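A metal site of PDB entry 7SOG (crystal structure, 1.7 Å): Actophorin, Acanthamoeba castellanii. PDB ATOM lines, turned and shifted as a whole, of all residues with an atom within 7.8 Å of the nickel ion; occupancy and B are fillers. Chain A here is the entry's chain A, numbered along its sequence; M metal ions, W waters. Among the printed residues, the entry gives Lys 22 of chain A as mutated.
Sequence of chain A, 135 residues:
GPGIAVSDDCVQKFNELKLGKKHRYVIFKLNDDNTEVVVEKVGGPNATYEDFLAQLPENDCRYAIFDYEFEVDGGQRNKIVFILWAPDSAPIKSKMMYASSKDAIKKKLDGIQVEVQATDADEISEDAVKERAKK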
ATOM      1  N   GLN A  12      25.332   6.737 -23.272  1.00  0.00           N
ATOM      2  CA  GLN A  12      25.178   7.956 -24.055  1.00  0.00           C
ATOM      3  C   GLN A  12      24.413   9.015 -23.261  1.00  0.00           C
ATOM      4  O   GLN A  12      24.825  10.170 -23.171  1.00  0.00           O
ATOM      5  CB  GLN A  12      24.482   7.610 -25.368  1.00  0.00           C
ATOM      6  CG  GLN A  12      23.979   8.764 -26.209  1.00  0.00           C
ATOM      7  CD  GLN A  12      22.956   8.295 -27.249  1.00  0.00           C
ATOM      8  OE1 GLN A  12      21.994   7.587 -26.914  1.00  0.00           O
ATOM      9  NE2 GLN A  12      23.159   8.672 -28.501  1.00  0.00           N
ATOM     10  N   LYS A  13      23.304   8.610 -22.634  1.00  0.00           N
ATOM     11  CA  LYS A  13      22.519   9.574 -21.861  1.00  0.00           C
ATOM     12  C   LYS A  13      23.214   9.933 -20.552  1.00  0.00           C
ATOM     13  O   LYS A  13      23.120  11.084 -20.115  1.00  0.00           O
ATOM     14  CB  LYS A  13      21.128   9.006 -21.590  1.00  0.00           C
ATOM     15  CG  LYS A  13      20.214   9.088 -22.789  1.00  0.00           C
ATOM     16  CD  LYS A  13      19.719  10.527 -22.997  1.00  0.00           C
ATOM     17  CE  LYS A  13      19.994  11.006 -24.402  1.00  0.00           C
ATOM     18  NZ  LYS A  13      19.156  12.194 -24.734  1.00  0.00           N
ATOM     19  N   GLU A  16      25.708  12.593 -21.418  1.00  0.00           N
ATOM     20  CA  GLU A  16      24.999  13.864 -21.603  1.00  0.00           C
ATOM     21  C   GLU A  16      24.744  14.542 -20.259  1.00  0.00           C
ATOM     22  O   GLU A  16      24.837  15.768 -20.134  1.00  0.00           O
ATOM     23  CB  GLU A  16      23.679  13.641 -22.341  1.00  0.00           C
ATOM     24  CG  GLU A  16      23.843  13.387 -23.834  1.00  0.00           C
ATOM     25  CD  GLU A  16      22.522  13.368 -24.575  1.00  0.00           C
ATOM     26  OE1 GLU A  16      21.500  13.927 -24.090  1.00  0.00           O
ATOM     27  OE2 GLU A  16      22.488  12.766 -25.678  1.00  0.00           O
ATOM     28  N   LEU A  17      24.435  13.757 -19.229  1.00  0.00           N
ATOM     29  CA  LEU A  17      24.211  14.308 -17.901  1.00  0.00           C
ATOM     30  C   LEU A  17      25.535  14.708 -17.245  1.00  0.00           C
ATOM     31  O   LEU A  17      25.676  15.847 -16.766  1.00  0.00           O
ATOM     32  CB  LEU A  17      23.463  13.299 -17.033  1.00  0.00           C
ATOM     33  CG  LEU A  17      23.232  13.613 -15.551  1.00  0.00           C
ATOM     34  CD1 LEU A  17      21.957  12.925 -15.093  1.00  0.00           C
ATOM     35  CD2 LEU A  17      24.416  13.182 -14.704  1.00  0.00           C
ATOM     36  N   LYS A  22      23.006  18.271 -19.624  1.00  0.00           N
ATOM     37  CA  LYS A  22      21.860  18.346 -20.519  1.00  0.00           C
ATOM     38  C   LYS A  22      20.599  17.749 -19.920  1.00  0.00           C
ATOM     39  O   LYS A  22      19.490  18.034 -20.392  1.00  0.00           O
ATOM     40  CB  LYS A  22      22.133  17.585 -21.822  1.00  0.00           C
ATOM     41  CG  LYS A  22      23.128  18.227 -22.775  1.00  0.00           C
ATOM     42  CD  LYS A  22      23.262  17.406 -24.049  1.00  0.00           C
ATOM     43  CE  LYS A  22      21.967  17.338 -24.869  1.00  0.00           C
ATOM     44  NZ  LYS A  22      20.916  16.395 -24.351  1.00  0.00           N
ATOM     45  N   HIS A  23      20.740  16.886 -18.923  1.00  0.00           N
ATOM     46  CA  HIS A  23      19.617  16.188 -18.318  1.00  0.00           C
ATOM     47  C   HIS A  23      19.867  16.166 -16.827  1.00  0.00           C
ATOM     48  O   HIS A  23      20.994  15.871 -16.398  1.00  0.00           O
ATOM     49  CB  HIS A  23      19.500  14.766 -18.873  1.00  0.00           C
ATOM     50  CG  HIS A  23      19.144  14.720 -20.320  1.00  0.00           C
ATOM     51  ND1 HIS A  23      17.897  15.092 -20.794  1.00  0.00           N
ATOM     52  CD2 HIS A  23      19.863  14.365 -21.407  1.00  0.00           C
ATOM     53  CE1 HIS A  23      17.871  14.946 -22.112  1.00  0.00           C
ATOM     54  NE2 HIS A  23      19.055  14.517 -22.502  1.00  0.00           N
ATOM     55  N   VAL A  42      14.147  10.296 -19.219  1.00  0.00           N
ATOM     56  CA  VAL A  42      15.160  11.306 -18.925  1.00  0.00           C
ATOM     57  C   VAL A  42      14.462  12.601 -18.554  1.00  0.00           C
ATOM     58  O   VAL A  42      13.337  12.885 -19.001  1.00  0.00           O
ATOM     59  CB  VAL A  42      16.144  11.523 -20.098  1.00  0.00           C
ATOM     60  CG1 VAL A  42      16.904  10.236 -20.423  1.00  0.00           C
ATOM     61  CG2 VAL A  42      15.418  12.066 -21.311  1.00  0.00           C
ATOM     62  N   GLY A  43      15.121  13.394 -17.730  1.00  0.00           N
ATOM     63  CA  GLY A  43      14.591  14.664 -17.296  1.00  0.00           C
ATOM     64  C   GLY A  43      15.278  15.801 -18.057  1.00  0.00           C
ATOM     65  O   GLY A  43      16.393  15.660 -18.532  1.00  0.00           O
HETATM   66 NI    NI M   1      19.568  14.068 -24.505  1.00  0.00          NI
HETATM   67  O   HOH W   1      17.734  14.138 -24.934  1.00  0.00           O
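The backbone carbonyl oxygen of Glu 16 sits at hydrogen-bond distance from the backbone NH of Lys 22 (3.1 Å).
A ring nitrogen (NE2) of His 23 sits close to the side-chain amino group of Lys 22 (3.2 Å).
ND1 of His 23 sits at hydrogen-bond distance from O of Gly 43 (2.8 Å).
The nickel ion is bound by water W1 (1.9 Å), the side-chain amino group of Lys 13 (1.9 Å), the side-chain carboxylate of Glu 16 (2.0 Å) and a ring nitrogen (NE2) of His 23 (2.1 Å).
Slightly farther from the nickel ion lies NZ of Lys 22 (2.7 Å).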
